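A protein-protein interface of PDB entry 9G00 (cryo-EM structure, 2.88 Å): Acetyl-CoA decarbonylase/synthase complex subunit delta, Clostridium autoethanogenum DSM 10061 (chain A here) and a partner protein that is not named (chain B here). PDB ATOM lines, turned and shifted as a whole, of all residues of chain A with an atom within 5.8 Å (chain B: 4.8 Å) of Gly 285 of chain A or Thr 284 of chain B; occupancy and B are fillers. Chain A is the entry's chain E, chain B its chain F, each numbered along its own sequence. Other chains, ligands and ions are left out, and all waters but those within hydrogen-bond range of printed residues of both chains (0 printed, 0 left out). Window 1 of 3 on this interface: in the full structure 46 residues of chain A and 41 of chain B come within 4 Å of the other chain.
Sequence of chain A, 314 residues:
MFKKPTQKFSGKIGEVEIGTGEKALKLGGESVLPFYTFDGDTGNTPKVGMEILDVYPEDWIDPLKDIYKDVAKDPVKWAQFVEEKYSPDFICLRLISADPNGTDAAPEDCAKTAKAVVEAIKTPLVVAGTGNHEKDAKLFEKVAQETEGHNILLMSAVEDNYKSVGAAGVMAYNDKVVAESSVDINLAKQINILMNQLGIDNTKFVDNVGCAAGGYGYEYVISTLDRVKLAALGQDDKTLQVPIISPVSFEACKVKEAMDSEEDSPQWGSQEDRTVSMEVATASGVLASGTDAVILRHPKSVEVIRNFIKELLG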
ATOM      1  N   TYR A 218      35.788  18.907 -19.177  1.00  0.00           N
ATOM      2  CA  TYR A 218      35.232  19.737 -18.118  1.00  0.00           C
ATOM      3  C   TYR A 218      35.157  18.987 -16.795  1.00  0.00           C
ATOM      4  O   TYR A 218      35.429  19.567 -15.740  1.00  0.00           O
ATOM      5  CB  TYR A 218      33.850  20.233 -18.536  1.00  0.00           C
ATOM      6  CG  TYR A 218      33.293  21.331 -17.676  1.00  0.00           C
ATOM      7  CD1 TYR A 218      33.893  22.578 -17.643  1.00  0.00           C
ATOM      8  CD2 TYR A 218      32.155  21.131 -16.914  1.00  0.00           C
ATOM      9  CE1 TYR A 218      33.384  23.587 -16.869  1.00  0.00           C
ATOM     10  CE2 TYR A 218      31.640  22.135 -16.137  1.00  0.00           C
ATOM     11  CZ  TYR A 218      32.260  23.361 -16.120  1.00  0.00           C
ATOM     12  OH  TYR A 218      31.750  24.364 -15.346  1.00  0.00           O
ATOM     13  N   ILE A 222      36.090  19.890 -12.794  1.00  0.00           N
ATOM     14  CA  ILE A 222      35.089  19.805 -11.735  1.00  0.00           C
ATOM     15  C   ILE A 222      35.581  18.913 -10.604  1.00  0.00           C
ATOM     16  O   ILE A 222      35.436  19.248  -9.424  1.00  0.00           O
ATOM     17  CB  ILE A 222      33.750  19.309 -12.315  1.00  0.00           C
ATOM     18  CG1 ILE A 222      33.193  20.320 -13.322  1.00  0.00           C
ATOM     19  CG2 ILE A 222      32.739  19.041 -11.215  1.00  0.00           C
ATOM     20  CD1 ILE A 222      32.981  21.711 -12.776  1.00  0.00           C
ATOM     21  N   LEU A 225      38.341  20.710  -8.613  1.00  0.00           N
ATOM     22  CA  LEU A 225      37.800  21.748  -7.745  1.00  0.00           C
ATOM     23  C   LEU A 225      37.107  21.146  -6.531  1.00  0.00           C
ATOM     24  O   LEU A 225      37.250  21.650  -5.413  1.00  0.00           O
ATOM     25  CB  LEU A 225      36.838  22.634  -8.529  1.00  0.00           C
ATOM     26  CG  LEU A 225      37.493  23.663  -9.448  1.00  0.00           C
ATOM     27  CD1 LEU A 225      36.466  24.278 -10.358  1.00  0.00           C
ATOM     28  CD2 LEU A 225      38.175  24.737  -8.636  1.00  0.00           C
ATOM     29  N   VAL A 280      28.527  31.351 -19.714  1.00  0.00           N
ATOM     30  CA  VAL A 280      27.664  31.295 -18.539  1.00  0.00           C
ATOM     31  C   VAL A 280      27.602  29.874 -17.998  1.00  0.00           C
ATOM     32  O   VAL A 280      27.660  29.653 -16.785  1.00  0.00           O
ATOM     33  CB  VAL A 280      26.268  31.844 -18.880  1.00  0.00           C
ATOM     34  CG1 VAL A 280      25.312  31.614 -17.738  1.00  0.00           C
ATOM     35  CG2 VAL A 280      26.353  33.322 -19.179  1.00  0.00           C
ATOM     36  N   ALA A 281      27.457  28.888 -18.883  1.00  0.00           N
ATOM     37  CA  ALA A 281      27.429  27.502 -18.432  1.00  0.00           C
ATOM     38  C   ALA A 281      28.759  27.096 -17.814  1.00  0.00           C
ATOM     39  O   ALA A 281      28.790  26.436 -16.770  1.00  0.00           O
ATOM     40  CB  ALA A 281      27.081  26.578 -19.596  1.00  0.00           C
ATOM     41  N   THR A 282      29.869  27.474 -18.443  1.00  0.00           N
ATOM     42  CA  THR A 282      31.176  27.113 -17.907  1.00  0.00           C
ATOM     43  C   THR A 282      31.440  27.801 -16.573  1.00  0.00           C
ATOM     44  O   THR A 282      31.947  27.174 -15.638  1.00  0.00           O
ATOM     45  CB  THR A 282      32.267  27.473 -18.912  1.00  0.00           C
ATOM     46  OG1 THR A 282      31.957  26.887 -20.181  1.00  0.00           O
ATOM     47  CG2 THR A 282      33.616  26.962 -18.447  1.00  0.00           C
ATOM     48  N   ALA A 283      31.105  29.086 -16.466  1.00  0.00           N
ATOM     49  CA  ALA A 283      31.404  29.831 -15.247  1.00  0.00           C
ATOM     50  C   ALA A 283      30.526  29.388 -14.087  1.00  0.00           C
ATOM     51  O   ALA A 283      30.996  29.290 -12.949  1.00  0.00           O
ATOM     52  CB  ALA A 283      31.238  31.326 -15.498  1.00  0.00           C
ATOM     53  N   SER A 284      29.246  29.129 -14.347  1.00  0.00           N
ATOM     54  CA  SER A 284      28.344  28.726 -13.274  1.00  0.00           C
ATOM     55  C   SER A 284      28.759  27.383 -12.689  1.00  0.00           C
ATOM     56  O   SER A 284      28.654  27.166 -11.478  1.00  0.00           O
ATOM     57  CB  SER A 284      26.910  28.675 -13.787  1.00  0.00           C
ATOM     58  OG  SER A 284      26.794  27.763 -14.856  1.00  0.00           O
ATOM     59  N   GLY A 285      29.205  26.460 -13.537  1.00  0.00           N
ATOM     60  CA  GLY A 285      29.619  25.158 -13.045  1.00  0.00           C
ATOM     61  C   GLY A 285      30.888  25.210 -12.212  1.00  0.00           C
ATOM     62  O   GLY A 285      31.024  24.473 -11.234  1.00  0.00           O
ATOM     63  N   VAL A 286      31.851  26.043 -12.607  1.00  0.00           N
ATOM     64  CA  VAL A 286      33.081  26.135 -11.823  1.00  0.00           C
ATOM     65  C   VAL A 286      32.856  26.952 -10.555  1.00  0.00           C
ATOM     66  O   VAL A 286      33.532  26.730  -9.547  1.00  0.00           O
ATOM     67  CB  VAL A 286      34.234  26.715 -12.659  1.00  0.00           C
ATOM     68  CG1 VAL A 286      34.497  25.843 -13.865  1.00  0.00           C
ATOM     69  CG2 VAL A 286      33.938  28.130 -13.084  1.00  0.00           C
ATOM     70  N   LEU A 287      31.921  27.906 -10.577  1.00  0.00           N
ATOM     71  CA  LEU A 287      31.596  28.640  -9.359  1.00  0.00           C
ATOM     72  C   LEU A 287      30.994  27.719  -8.308  1.00  0.00           C
ATOM     73  O   LEU A 287      31.313  27.831  -7.120  1.00  0.00           O
ATOM     74  CB  LEU A 287      30.637  29.789  -9.666  1.00  0.00           C
ATOM     75  CG  LEU A 287      31.245  31.053 -10.271  1.00  0.00           C
ATOM     76  CD1 LEU A 287      30.149  32.027 -10.632  1.00  0.00           C
ATOM     77  CD2 LEU A 287      32.236  31.708  -9.320  1.00  0.00           C
ATOM     78  N   ALA A 288      30.115  26.807  -8.724  1.00  0.00           N
ATOM     79  CA  ALA A 288      29.517  25.880  -7.775  1.00  0.00           C
ATOM     80  C   ALA A 288      30.516  24.864  -7.244  1.00  0.00           C
ATOM     81  O   ALA A 288      30.240  24.225  -6.225  1.00  0.00           O
ATOM     82  CB  ALA A 288      28.345  25.150  -8.427  1.00  0.00           C
ATOM     83  N   SER A 289      31.650  24.677  -7.918  1.00  0.00           N
ATOM     84  CA  SER A 289      32.634  23.686  -7.507  1.00  0.00           C
ATOM     85  C   SER A 289      33.732  24.244  -6.612  1.00  0.00           C
ATOM     86  O   SER A 289      34.491  23.456  -6.041  1.00  0.00           O
ATOM     87  CB  SER A 289      33.279  23.049  -8.735  1.00  0.00           C
ATOM     88  OG  SER A 289      32.319  22.332  -9.484  1.00  0.00           O
ATOM     89  N   GLY A 290      33.823  25.562  -6.446  1.00  0.00           N
ATOM     90  CA  GLY A 290      34.811  26.119  -5.542  1.00  0.00           C
ATOM     91  C   GLY A 290      35.762  27.146  -6.126  1.00  0.00           C
ATOM     92  O   GLY A 290      36.876  27.307  -5.624  1.00  0.00           O
ATOM     93  N   VAL B 280      20.244  28.498 -18.485  1.00  0.00           N
ATOM     94  CA  VAL B 280      21.453  27.709 -18.725  1.00  0.00           C
ATOM     95  C   VAL B 280      22.323  27.658 -17.466  1.00  0.00           C
ATOM     96  O   VAL B 280      22.863  26.601 -17.105  1.00  0.00           O
ATOM     97  CB  VAL B 280      22.222  28.256 -19.943  1.00  0.00           C
ATOM     98  CG1 VAL B 280      22.622  29.692 -19.733  1.00  0.00           C
ATOM     99  CG2 VAL B 280      23.443  27.406 -20.231  1.00  0.00           C
ATOM    100  N   ALA B 281      22.463  28.790 -16.772  1.00  0.00           N
ATOM    101  CA  ALA B 281      23.276  28.822 -15.558  1.00  0.00           C
ATOM    102  C   ALA B 281      22.703  27.905 -14.484  1.00  0.00           C
ATOM    103  O   ALA B 281      23.425  27.102 -13.879  1.00  0.00           O
ATOM    104  CB  ALA B 281      23.378  30.253 -15.036  1.00  0.00           C
ATOM    105  N   LEU B 282      21.400  28.015 -14.226  1.00  0.00           N
ATOM    106  CA  LEU B 282      20.791  27.172 -13.204  1.00  0.00           C
ATOM    107  C   LEU B 282      20.772  25.708 -13.620  1.00  0.00           C
ATOM    108  O   LEU B 282      20.861  24.824 -12.763  1.00  0.00           O
ATOM    109  CB  LEU B 282      19.380  27.652 -12.886  1.00  0.00           C
ATOM    110  CG  LEU B 282      19.256  28.962 -12.107  1.00  0.00           C
ATOM    111  CD1 LEU B 282      17.829  29.121 -11.644  1.00  0.00           C
ATOM    112  CD2 LEU B 282      20.204  29.030 -10.917  1.00  0.00           C
ATOM    113  N   SER B 283      20.653  25.429 -14.917  1.00  0.00           N
ATOM    114  CA  SER B 283      20.706  24.050 -15.380  1.00  0.00           C
ATOM    115  C   SER B 283      22.069  23.439 -15.109  1.00  0.00           C
ATOM    116  O   SER B 283      22.159  22.292 -14.667  1.00  0.00           O
ATOM    117  CB  SER B 283      20.378  23.988 -16.868  1.00  0.00           C
ATOM    118  OG  SER B 283      19.128  24.591 -17.137  1.00  0.00           O
ATOM    119  N   THR B 284      23.142  24.187 -15.358  1.00  0.00           N
ATOM    120  CA  THR B 284      24.468  23.692 -14.993  1.00  0.00           C
ATOM    121  C   THR B 284      24.575  23.481 -13.485  1.00  0.00           C
ATOM    122  O   THR B 284      25.053  22.434 -13.015  1.00  0.00           O
ATOM    123  CB  THR B 284      25.536  24.670 -15.472  1.00  0.00           C
ATOM    124  OG1 THR B 284      25.312  24.984 -16.849  1.00  0.00           O
ATOM    125  CG2 THR B 284      26.912  24.069 -15.321  1.00  0.00           C
ATOM    126  N   LEU B 285      24.106  24.459 -12.711  1.00  0.00           N
ATOM    127  CA  LEU B 285      24.194  24.360 -11.258  1.00  0.00           C
ATOM    128  C   LEU B 285      23.517  23.093 -10.749  1.00  0.00           C
ATOM    129  O   LEU B 285      24.086  22.358  -9.937  1.00  0.00           O
ATOM    130  CB  LEU B 285      23.564  25.596 -10.621  1.00  0.00           C
ATOM    131  CG  LEU B 285      23.412  25.571  -9.101  1.00  0.00           C
ATOM    132  CD1 LEU B 285      24.769  25.616  -8.432  1.00  0.00           C
ATOM    133  CD2 LEU B 285      22.543  26.725  -8.649  1.00  0.00           C
ATOM    134  N   PHE B 286      22.293  22.826 -11.207  1.00  0.00           N
ATOM    135  CA  PHE B 286      21.547  21.668 -10.729  1.00  0.00           C
ATOM    136  C   PHE B 286      21.947  20.374 -11.421  1.00  0.00           C
ATOM    137  O   PHE B 286      21.573  19.299 -10.944  1.00  0.00           O
ATOM    138  CB  PHE B 286      20.047  21.899 -10.892  1.00  0.00           C
ATOM    139  CG  PHE B 286      19.495  22.928  -9.954  1.00  0.00           C
ATOM    140  CD1 PHE B 286      19.443  22.688  -8.597  1.00  0.00           C
ATOM    141  CD2 PHE B 286      19.025  24.135 -10.429  1.00  0.00           C
ATOM    142  CE1 PHE B 286      18.938  23.633  -7.736  1.00  0.00           C
ATOM    143  CE2 PHE B 286      18.517  25.080  -9.568  1.00  0.00           C
ATOM    144  CZ  PHE B 286      18.473  24.828  -8.223  1.00  0.00           C
ATOM    145  N   THR B 287      22.661  20.443 -12.545  1.00  0.00           N
ATOM    146  CA  THR B 287      23.333  19.257 -13.055  1.00  0.00           C
ATOM    147  C   THR B 287      24.424  18.815 -12.097  1.00  0.00           C
ATOM    148  O   THR B 287      24.615  17.617 -11.872  1.00  0.00           O
ATOM    149  CB  THR B 287      23.929  19.535 -14.434  1.00  0.00           C
ATOM    150  OG1 THR B 287      22.886  19.876 -15.354  1.00  0.00           O
ATOM    151  CG2 THR B 287      24.679  18.322 -14.957  1.00  0.00           C
ATOM    152  N   LEU B 288      25.158  19.773 -11.531  1.00  0.00           N
ATOM    153  CA  LEU B 288      26.188  19.432 -10.561  1.00  0.00           C
ATOM    154  C   LEU B 288      25.672  19.321  -9.133  1.00  0.00           C
ATOM    155  O   LEU B 288      26.416  18.861  -8.263  1.00  0.00           O
ATOM    156  CB  LEU B 288      27.312  20.472 -10.604  1.00  0.00           C
ATOM    157  CG  LEU B 288      28.204  20.426 -11.841  1.00  0.00           C
ATOM    158  CD1 LEU B 288      29.118  21.625 -11.874  1.00  0.00           C
ATOM    159  CD2 LEU B 288      29.014  19.149 -11.856  1.00  0.00           C
ATOM    160  N   LEU B 307      24.686  22.649 -22.213  1.00  0.00           N
ATOM    161  CA  LEU B 307      24.076  21.818 -21.180  1.00  0.00           C
ATOM    162  C   LEU B 307      24.262  20.334 -21.466  1.00  0.00           C
ATOM    163  O   LEU B 307      24.535  19.554 -20.548  1.00  0.00           O
ATOM    164  CB  LEU B 307      22.594  22.154 -21.044  1.00  0.00           C
ATOM    165  CG  LEU B 307      22.286  23.571 -20.556  1.00  0.00           C
ATOM    166  CD1 LEU B 307      20.790  23.764 -20.420  1.00  0.00           C
ATOM    167  CD2 LEU B 307      22.975  23.868 -19.238  1.00  0.00           C
ATOM    168  N   ILE B 310      28.110  19.472 -21.142  1.00  0.00           N
ATOM    169  CA  ILE B 310      28.525  19.403 -19.745  1.00  0.00           C
ATOM    170  C   ILE B 310      27.976  18.144 -19.092  1.00  0.00           C
ATOM    171  O   ILE B 310      28.682  17.459 -18.341  1.00  0.00           O
ATOM    172  CB  ILE B 310      28.088  20.674 -18.994  1.00  0.00           C
ATOM    173  CG1 ILE B 310      28.935  21.860 -19.457  1.00  0.00           C
ATOM    174  CG2 ILE B 310      28.201  20.480 -17.479  1.00  0.00           C
ATOM    175  CD1 ILE B 310      28.589  23.167 -18.804  1.00  0.00           C
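Of the printed residues of chain B, Ala 288 of chain A touches Leu 285 (3.6 Å).
Of the printed residues of chain A, Ala 281 of chain B touches Val 280 (3.6 Å) and Ser 284 (3.6 Å).
Ser 283 of chain B touches none of the printed residues of chain A.
Printed residues of chain A within 4 Å of Leu 285 of chain B: Ala 288.
The nearest printed residue of chain B that does not touch Gly 285 of chain A is Leu 285 of chain B (5.5 Å).
The nearest printed residue of chain B that does not touch Ile 222 of chain A is Ile 310 of chain B (6.5 Å).
O of Gly 285 of chain A lies within hydrogen-bond range of OG of Ser 289 of chain A.
The backbone carbonyl oxygen (O) of Val 280 of chain A sits at hydrogen-bond distance from the side-chain hydroxyl (OG) of Ser 284 of chain A (2.8 Å).
O of Val 280 of chain B is in hydrogen-bond range of OG1 of Thr 284 of chain B (2.9 Å).
The backbone carbonyl oxygen (O) of Ala 281 of chain A is in hydrogen-bond range of the side-chain hydroxyl (OG) of Ser 284 of chain A (3.1 Å).
Among the printed residues, pairs that only touch across the chains: Ile 222 of chain A with Leu 288 of chain B (3.8 Å), Val 280 of chain A with Val 280 of chain B (3.9 Å), Val 280 of chain A with Ala 281 of chain B (3.6 Å), Ala 281 of chain A with Val 280 of chain B (3.8 Å), Ala 281 of chain A with Thr 284 of chain B (3.4 Å), Ala 281 of chain A with Ile 310 of chain B (3.8 Å), Ser 284 of chain A with Ala 281 of chain B (3.6 Å), Ser 284 of chain A with Thr 284 of chain B (3.4 Å), Gly 285 of chain A with Thr 284 of chain B (3.7 Å), Gly 285 of chain A with Leu 288 of chain B (3.5 Å) and Ala 288 of chain A with Leu 285 of chain B (3.6 Å).
Of the 14 printed residues of chain A, 6 touch a printed residue of chain B.
Hydrophobic or aromatic side chains of chain B that line the printed part of chain A: Val 280, Ala 281, Leu 285, Leu 288 and Ile 310.
Among the printed residues, 11 pairs touch across the chains.
Among the printed residues, no Asp or Glu carboxylate lies within 4 Å of a Lys or Arg side-chain nitrogen of the other chain.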
